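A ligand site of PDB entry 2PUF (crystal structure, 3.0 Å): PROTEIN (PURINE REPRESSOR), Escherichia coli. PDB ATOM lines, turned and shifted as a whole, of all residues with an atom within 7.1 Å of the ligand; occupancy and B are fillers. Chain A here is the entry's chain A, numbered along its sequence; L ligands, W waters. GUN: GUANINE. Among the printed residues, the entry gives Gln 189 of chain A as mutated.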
ATOM      1  N   THR A  66      -2.105  11.105  12.995  1.00  0.00           N
ATOM      2  CA  THR A  66      -1.771  11.988  11.898  1.00  0.00           C
ATOM      3  C   THR A  66      -1.180  11.175  10.744  1.00  0.00           C
ATOM      4  O   THR A  66      -1.512  11.380   9.577  1.00  0.00           O
ATOM      5  CB  THR A  66      -0.750  13.006  12.339  1.00  0.00           C
ATOM      6  OG1 THR A  66      -1.425  14.158  12.856  1.00  0.00           O
ATOM      7  CG2 THR A  66       0.112  13.425  11.184  1.00  0.00           C
ATOM      8  N   SER A  67      -0.330  10.227  11.096  1.00  0.00           N
ATOM      9  CA  SER A  67       0.309   9.353  10.122  1.00  0.00           C
ATOM     10  C   SER A  67       0.923   8.199  10.915  1.00  0.00           C
ATOM     11  O   SER A  67       1.119   8.312  12.125  1.00  0.00           O
ATOM     12  CB  SER A  67       1.374  10.135   9.339  1.00  0.00           C
ATOM     13  OG  SER A  67       2.447   9.294   8.977  1.00  0.00           O
ATOM     14  N   ALA A  70       6.144   7.565  10.081  1.00  0.00           N
ATOM     15  CA  ALA A  70       7.214   8.296  10.734  1.00  0.00           C
ATOM     16  C   ALA A  70       7.616   7.566  12.009  1.00  0.00           C
ATOM     17  O   ALA A  70       6.761   7.214  12.822  1.00  0.00           O
ATOM     18  CB  ALA A  70       6.770   9.706  11.040  1.00  0.00           C
ATOM     19  N   ALA A  71       8.903   7.314  12.169  1.00  0.00           N
ATOM     20  CA  ALA A  71       9.425   6.610  13.332  1.00  0.00           C
ATOM     21  C   ALA A  71       8.804   7.070  14.635  1.00  0.00           C
ATOM     22  O   ALA A  71       8.360   6.258  15.447  1.00  0.00           O
ATOM     23  CB  ALA A  71      10.934   6.724  13.385  1.00  0.00           C
ATOM     24  N   TYR A  72       8.782   8.389  14.823  1.00  0.00           N
ATOM     25  CA  TYR A  72       8.221   8.984  16.012  1.00  0.00           C
ATOM     26  C   TYR A  72       6.826   8.399  16.280  1.00  0.00           C
ATOM     27  O   TYR A  72       6.608   7.740  17.287  1.00  0.00           O
ATOM     28  CB  TYR A  72       8.135  10.506  15.836  1.00  0.00           C
ATOM     29  CG  TYR A  72       7.648  11.247  17.063  1.00  0.00           C
ATOM     30  CD1 TYR A  72       8.509  11.548  18.102  1.00  0.00           C
ATOM     31  CD2 TYR A  72       6.323  11.636  17.180  1.00  0.00           C
ATOM     32  CE1 TYR A  72       8.059  12.242  19.235  1.00  0.00           C
ATOM     33  CE2 TYR A  72       5.874  12.319  18.304  1.00  0.00           C
ATOM     34  CZ  TYR A  72       6.744  12.612  19.322  1.00  0.00           C
ATOM     35  OH  TYR A  72       6.291  13.292  20.416  1.00  0.00           O
ATOM     36  N   PHE A  73       5.928   8.601  15.343  1.00  0.00           N
ATOM     37  CA  PHE A  73       4.585   8.096  15.483  1.00  0.00           C
ATOM     38  C   PHE A  73       4.547   6.583  15.677  1.00  0.00           C
ATOM     39  O   PHE A  73       4.022   6.090  16.676  1.00  0.00           O
ATOM     40  CB  PHE A  73       3.773   8.461  14.264  1.00  0.00           C
ATOM     41  CG  PHE A  73       3.594   9.927  14.076  1.00  0.00           C
ATOM     42  CD1 PHE A  73       3.479  10.759  15.166  1.00  0.00           C
ATOM     43  CD2 PHE A  73       3.539  10.460  12.818  1.00  0.00           C
ATOM     44  CE1 PHE A  73       3.313  12.105  14.998  1.00  0.00           C
ATOM     45  CE2 PHE A  73       3.372  11.805  12.640  1.00  0.00           C
ATOM     46  CZ  PHE A  73       3.269  12.630  13.728  1.00  0.00           C
ATOM     47  N   SER A 123      -1.635  16.615  15.651  1.00  0.00           N
ATOM     48  CA  SER A 123      -0.554  17.561  15.379  1.00  0.00           C
ATOM     49  C   SER A 123      -1.034  18.988  15.384  1.00  0.00           C
ATOM     50  O   SER A 123      -0.867  19.703  16.360  1.00  0.00           O
ATOM     51  CB  SER A 123       0.122  17.209  14.068  1.00  0.00           C
ATOM     52  OG  SER A 123       0.533  15.858  14.077  1.00  0.00           O
ATOM     53  N   ASP A 145      -0.679  14.743  22.196  1.00  0.00           N
ATOM     54  CA  ASP A 145       0.395  15.548  21.623  1.00  0.00           C
ATOM     55  C   ASP A 145       0.173  17.050  21.774  1.00  0.00           C
ATOM     56  O   ASP A 145       0.348  17.795  20.826  1.00  0.00           O
ATOM     57  CB  ASP A 145       0.559  15.196  20.137  1.00  0.00           C
ATOM     58  CG  ASP A 145      -0.666  15.584  19.284  1.00  0.00           C
ATOM     59  OD1 ASP A 145      -1.592  16.244  19.802  1.00  0.00           O
ATOM     60  OD2 ASP A 145      -0.683  15.229  18.079  1.00  0.00           O
ATOM     61  N   ASP A 159       4.306  16.739  27.345  1.00  0.00           N
ATOM     62  CA  ASP A 159       5.692  16.295  27.254  1.00  0.00           C
ATOM     63  C   ASP A 159       6.781  17.213  27.816  1.00  0.00           C
ATOM     64  O   ASP A 159       7.930  16.808  27.920  1.00  0.00           O
ATOM     65  CB  ASP A 159       6.025  15.886  25.818  1.00  0.00           C
ATOM     66  CG  ASP A 159       5.819  17.024  24.822  1.00  0.00           C
ATOM     67  OD1 ASP A 159       5.437  18.145  25.235  1.00  0.00           O
ATOM     68  OD2 ASP A 159       6.064  16.791  23.617  1.00  0.00           O
ATOM     69  N   PRO A 186       7.679  22.157  12.215  1.00  0.00           N
ATOM     70  CA  PRO A 186       6.551  23.089  11.989  1.00  0.00           C
ATOM     71  C   PRO A 186       6.039  23.794  13.253  1.00  0.00           C
ATOM     72  O   PRO A 186       5.757  23.149  14.279  1.00  0.00           O
ATOM     73  CB  PRO A 186       5.473  22.174  11.435  1.00  0.00           C
ATOM     74  CG  PRO A 186       5.763  20.844  12.090  1.00  0.00           C
ATOM     75  CD  PRO A 186       7.260  20.749  12.184  1.00  0.00           C
ATOM     76  N   GLN A 189       2.817  23.062  15.296  1.00  0.00           N
ATOM     77  CA  GLN A 189       2.957  21.923  16.211  1.00  0.00           C
ATOM     78  C   GLN A 189       3.518  22.275  17.586  1.00  0.00           C
ATOM     79  O   GLN A 189       4.072  23.365  17.798  1.00  0.00           O
ATOM     80  CB  GLN A 189       3.841  20.862  15.583  1.00  0.00           C
ATOM     81  CG  GLN A 189       3.193  20.065  14.495  1.00  0.00           C
ATOM     82  CD  GLN A 189       3.587  18.631  14.586  1.00  0.00           C
ATOM     83  OE1 GLN A 189       3.517  17.881  13.629  1.00  0.00           O
ATOM     84  NE2 GLN A 189       4.051  18.244  15.759  1.00  0.00           N
ATOM     85  N   ASN A 190       3.391  21.314  18.496  1.00  0.00           N
ATOM     86  CA  ASN A 190       3.899  21.455  19.858  1.00  0.00           C
ATOM     87  C   ASN A 190       5.380  21.090  19.826  1.00  0.00           C
ATOM     88  O   ASN A 190       6.238  21.867  20.234  1.00  0.00           O
ATOM     89  CB  ASN A 190       3.160  20.476  20.771  1.00  0.00           C
ATOM     90  CG  ASN A 190       3.829  20.296  22.107  1.00  0.00           C
ATOM     91  OD1 ASN A 190       4.064  21.253  22.807  1.00  0.00           O
ATOM     92  ND2 ASN A 190       4.047  19.058  22.491  1.00  0.00           N
ATOM     93  N   THR A 191       5.656  19.905  19.313  1.00  0.00           N
ATOM     94  CA  THR A 191       7.006  19.407  19.171  1.00  0.00           C
ATOM     95  C   THR A 191       7.732  20.295  18.167  1.00  0.00           C
ATOM     96  O   THR A 191       8.949  20.183  17.960  1.00  0.00           O
ATOM     97  CB  THR A 191       6.981  17.996  18.643  1.00  0.00           C
ATOM     98  OG1 THR A 191       6.117  17.938  17.522  1.00  0.00           O
ATOM     99  CG2 THR A 191       6.477  17.056  19.700  1.00  0.00           C
ATOM    100  N   GLY A 192       6.973  21.180  17.532  1.00  0.00           N
ATOM    101  CA  GLY A 192       7.520  22.117  16.591  1.00  0.00           C
ATOM    102  C   GLY A 192       7.927  23.333  17.403  1.00  0.00           C
ATOM    103  O   GLY A 192       9.053  23.408  17.894  1.00  0.00           O
ATOM    104  N   ARG A 195       9.550  23.004  21.247  1.00  0.00           N
ATOM    105  CA  ARG A 195      10.964  22.682  21.375  1.00  0.00           C
ATOM    106  C   ARG A 195      11.832  23.920  21.027  1.00  0.00           C
ATOM    107  O   ARG A 195      12.716  24.307  21.791  1.00  0.00           O
ATOM    108  CB  ARG A 195      11.313  21.486  20.485  1.00  0.00           C
ATOM    109  CG  ARG A 195      10.654  20.194  20.927  1.00  0.00           C
ATOM    110  CD  ARG A 195      10.706  19.128  19.848  1.00  0.00           C
ATOM    111  NE  ARG A 195      10.351  17.807  20.368  1.00  0.00           N
ATOM    112  CZ  ARG A 195      10.389  16.683  19.662  1.00  0.00           C
ATOM    113  NH1 ARG A 195      10.764  16.678  18.397  1.00  0.00           N
ATOM    114  NH2 ARG A 195      10.060  15.548  20.243  1.00  0.00           N
ATOM    115  N   ASP A 219      10.044  19.850   8.436  1.00  0.00           N
ATOM    116  CA  ASP A 219       8.751  19.226   8.630  1.00  0.00           C
ATOM    117  C   ASP A 219       8.841  17.817   9.171  1.00  0.00           C
ATOM    118  O   ASP A 219       7.936  17.007   8.978  1.00  0.00           O
ATOM    119  CB  ASP A 219       7.947  19.269   7.348  1.00  0.00           C
ATOM    120  CG  ASP A 219       8.581  18.450   6.249  1.00  0.00           C
ATOM    121  OD1 ASP A 219       9.446  17.607   6.538  1.00  0.00           O
ATOM    122  OD2 ASP A 219       8.167  18.613   5.088  1.00  0.00           O
ATOM    123  N   PHE A 220       9.959  17.515   9.840  1.00  0.00           N
ATOM    124  CA  PHE A 220      10.190  16.186  10.403  1.00  0.00           C
ATOM    125  C   PHE A 220      10.559  15.153   9.333  1.00  0.00           C
ATOM    126  O   PHE A 220      10.884  14.011   9.631  1.00  0.00           O
ATOM    127  CB  PHE A 220       8.977  15.718  11.221  1.00  0.00           C
ATOM    128  CG  PHE A 220       8.794  16.459  12.502  1.00  0.00           C
ATOM    129  CD1 PHE A 220       9.865  16.643  13.377  1.00  0.00           C
ATOM    130  CD2 PHE A 220       7.566  16.990  12.845  1.00  0.00           C
ATOM    131  CE1 PHE A 220       9.702  17.322  14.570  1.00  0.00           C
ATOM    132  CE2 PHE A 220       7.402  17.680  14.047  1.00  0.00           C
ATOM    133  CZ  PHE A 220       8.476  17.842  14.903  1.00  0.00           C
ATOM    134  N   GLU A 221      10.534  15.570   8.080  1.00  0.00           N
ATOM    135  CA  GLU A 221      10.891  14.687   6.978  1.00  0.00           C
ATOM    136  C   GLU A 221      12.399  14.814   6.685  1.00  0.00           C
ATOM    137  O   GLU A 221      12.916  15.917   6.535  1.00  0.00           O
ATOM    138  CB  GLU A 221      10.073  15.019   5.733  1.00  0.00           C
ATOM    139  CG  GLU A 221       8.558  14.832   5.901  1.00  0.00           C
ATOM    140  CD  GLU A 221       8.154  13.350   5.966  1.00  0.00           C
ATOM    141  OE1 GLU A 221       8.435  12.599   4.985  1.00  0.00           O
ATOM    142  OE2 GLU A 221       7.536  12.947   6.981  1.00  0.00           O
ATOM    143  N   GLY A 245      15.438  19.965  15.004  1.00  0.00           N
ATOM    144  CA  GLY A 245      14.100  19.739  15.524  1.00  0.00           C
ATOM    145  C   GLY A 245      13.704  18.280  15.789  1.00  0.00           C
ATOM    146  O   GLY A 245      13.032  17.986  16.772  1.00  0.00           O
ATOM    147  N   GLY A 246      14.118  17.372  14.914  1.00  0.00           N
ATOM    148  CA  GLY A 246      13.777  15.954  15.075  1.00  0.00           C
ATOM    149  C   GLY A 246      14.911  15.012  14.672  1.00  0.00           C
ATOM    150  O   GLY A 246      15.828  15.396  13.958  1.00  0.00           O
ATOM    151  N   ASP A 247      14.828  13.770  15.123  1.00  0.00           N
ATOM    152  CA  ASP A 247      15.843  12.791  14.822  1.00  0.00           C
ATOM    153  C   ASP A 247      15.906  12.393  13.356  1.00  0.00           C
ATOM    154  O   ASP A 247      16.975  12.316  12.772  1.00  0.00           O
ATOM    155  CB  ASP A 247      15.659  11.563  15.673  1.00  0.00           C
ATOM    156  CG  ASP A 247      16.202  11.746  17.056  1.00  0.00           C
ATOM    157  OD1 ASP A 247      16.503  12.900  17.413  1.00  0.00           O
ATOM    158  OD2 ASP A 247      16.359  10.736  17.784  1.00  0.00           O
ATOM    159  N   ILE A 248      14.763  12.111  12.764  1.00  0.00           N
ATOM    160  CA  ILE A 248      14.714  11.707  11.366  1.00  0.00           C
ATOM    161  C   ILE A 248      15.060  12.860  10.436  1.00  0.00           C
ATOM    162  O   ILE A 248      15.376  12.669   9.278  1.00  0.00           O
ATOM    163  CB  ILE A 248      13.389  11.067  10.998  1.00  0.00           C
ATOM    164  CG1 ILE A 248      13.142   9.866  11.887  1.00  0.00           C
ATOM    165  CG2 ILE A 248      13.392  10.633   9.554  1.00  0.00           C
ATOM    166  CD1 ILE A 248      13.385   8.611  11.202  1.00  0.00           C
ATOM    167  N   TYR A 273      16.529  15.370  18.596  1.00  0.00           N
ATOM    168  CA  TYR A 273      15.468  15.366  19.582  1.00  0.00           C
ATOM    169  C   TYR A 273      14.415  14.402  19.161  1.00  0.00           C
ATOM    170  O   TYR A 273      13.722  14.635  18.180  1.00  0.00           O
ATOM    171  CB  TYR A 273      14.856  16.751  19.672  1.00  0.00           C
ATOM    172  CG  TYR A 273      13.961  16.978  20.865  1.00  0.00           C
ATOM    173  CD1 TYR A 273      13.174  15.955  21.384  1.00  0.00           C
ATOM    174  CD2 TYR A 273      13.885  18.220  21.465  1.00  0.00           C
ATOM    175  CE1 TYR A 273      12.341  16.182  22.456  1.00  0.00           C
ATOM    176  CE2 TYR A 273      13.065  18.439  22.536  1.00  0.00           C
ATOM    177  CZ  TYR A 273      12.290  17.430  23.031  1.00  0.00           C
ATOM    178  OH  TYR A 273      11.483  17.684  24.106  1.00  0.00           O
ATOM    179  N   ASP A 274      14.284  13.329  19.939  1.00  0.00           N
ATOM    180  CA  ASP A 274      13.288  12.268  19.762  1.00  0.00           C
ATOM    181  C   ASP A 274      13.781  10.969  20.363  1.00  0.00           C
ATOM    182  O   ASP A 274      13.056  10.284  21.075  1.00  0.00           O
ATOM    183  CB  ASP A 274      12.928  12.058  18.302  1.00  0.00           C
ATOM    184  CG  ASP A 274      11.682  12.836  17.894  1.00  0.00           C
ATOM    185  OD1 ASP A 274      11.167  13.591  18.747  1.00  0.00           O
ATOM    186  OD2 ASP A 274      11.289  12.776  16.711  1.00  0.00           O
ATOM    187  N   GLN A 291      12.455  11.446  24.281  1.00  0.00           N
ATOM    188  CA  GLN A 291      11.080  11.551  24.777  1.00  0.00           C
ATOM    189  C   GLN A 291      10.595  10.169  25.180  1.00  0.00           C
ATOM    190  O   GLN A 291      10.814   9.197  24.473  1.00  0.00           O
ATOM    191  CB  GLN A 291      10.171  12.105  23.698  1.00  0.00           C
ATOM    192  CG  GLN A 291       8.788  12.488  24.190  1.00  0.00           C
ATOM    193  CD  GLN A 291       8.361  13.873  23.723  1.00  0.00           C
ATOM    194  OE1 GLN A 291       7.721  14.014  22.681  1.00  0.00           O
ATOM    195  NE2 GLN A 291       8.761  14.908  24.472  1.00  0.00           N
HETATM  196  N9  GUN L   1       8.705  14.376  16.443  1.00  0.00           N
HETATM  197  C8  GUN L   1       7.918  15.071  17.323  1.00  0.00           C
HETATM  198  N7  GUN L   1       6.729  15.343  16.861  1.00  0.00           N
HETATM  199  C5  GUN L   1       6.730  14.792  15.591  1.00  0.00           C
HETATM  200  C6  GUN L   1       5.711  14.773  14.601  1.00  0.00           C
HETATM  201  O6  GUN L   1       4.575  15.251  14.671  1.00  0.00           O
HETATM  202  N1  GUN L   1       6.126  14.120  13.449  1.00  0.00           N
HETATM  203  C2  GUN L   1       7.362  13.549  13.271  1.00  0.00           C
HETATM  204  N2  GUN L   1       7.567  12.953  12.085  1.00  0.00           N
HETATM  205  N3  GUN L   1       8.316  13.558  14.180  1.00  0.00           N
HETATM  206  C4  GUN L   1       7.934  14.197  15.318  1.00  0.00           C
HETATM  207  O   HOH W   1       3.831  15.692  18.097  1.00  0.00           O
HETATM  208  O   HOH W   2       5.052  14.136  10.362  1.00  0.00           O
HETATM  209  O   HOH W   3       8.856  10.841  13.115  1.00  0.00           O
HETATM  210  O   HOH W   4       9.802  11.486  10.037  1.00  0.00           O
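Merely in contact with the ligand: Ala 70 (3.5 Å), Tyr 72 (3.3 Å), Phe 73 (3.1 Å), Arg 195 (3.4 Å) and Phe 220 (3.2 Å). Hydrophobic or aromatic side chains that line the ligand: Ala 70, Tyr 72, Phe 73 and Phe 220. Of the 25 residues printed, 8 come within 4 Å of the ligand. Along chain A the residues within 4 Å of the ligand span positions 70 to 274. The nearest printed residue that does not touch the ligand is Ser 123 (4.1 Å).
The side-chain amide nitrogen (NE2) of Gln 189 sits at hydrogen-bond distance from the side-chain hydroxyl (OG1) of Thr 191. The guanidinium group (NH2) of Arg 195 lies within salt-bridge range of the side-chain carboxylate (OD1) of Asp 274, at 2.7 Å. The backbone NH (N) of Gln 291 is in hydrogen-bond range of the backbone carbonyl oxygen (O) of Asp 274 (3.5 Å). The side-chain carboxylate of Asp 247 is in hydrogen-bond range of the backbone NH of Asp 274, at 3.4 Å. The side-chain hydroxyl of Tyr 72 sits at hydrogen-bond distance from the side-chain amide oxygen of Gln 291. The guanidinium group of Arg 195 sits at hydrogen-bond distance from the backbone carbonyl oxygen of Gly 245 (3.1 Å).
Water W3 bridges N2 of the ligand (2.7 Å) and N of Tyr 72 (3.0 Å). Water W1 lies within hydrogen-bond range of a nitrogen (N7) of the ligand (3.2 Å), the side-chain hydroxyl of Thr 191 (3.3 Å) and the side-chain amide nitrogen of Gln 189 (3.5 Å). Water W4 lies within hydrogen-bond range of the backbone carbonyl oxygen (O) of Phe 220 (2.8 Å) and a nitrogen (N2) of the ligand (3.4 Å).
OG1 of Thr 191 is in hydrogen-bond range of N7 of the ligand (2.7 Å). OE1 of Gln 189 sits close to O6 of the ligand (3.0 Å). OD2 of Asp 274 sits at hydrogen-bond distance from N9 of the ligand, at 3.1 Å.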
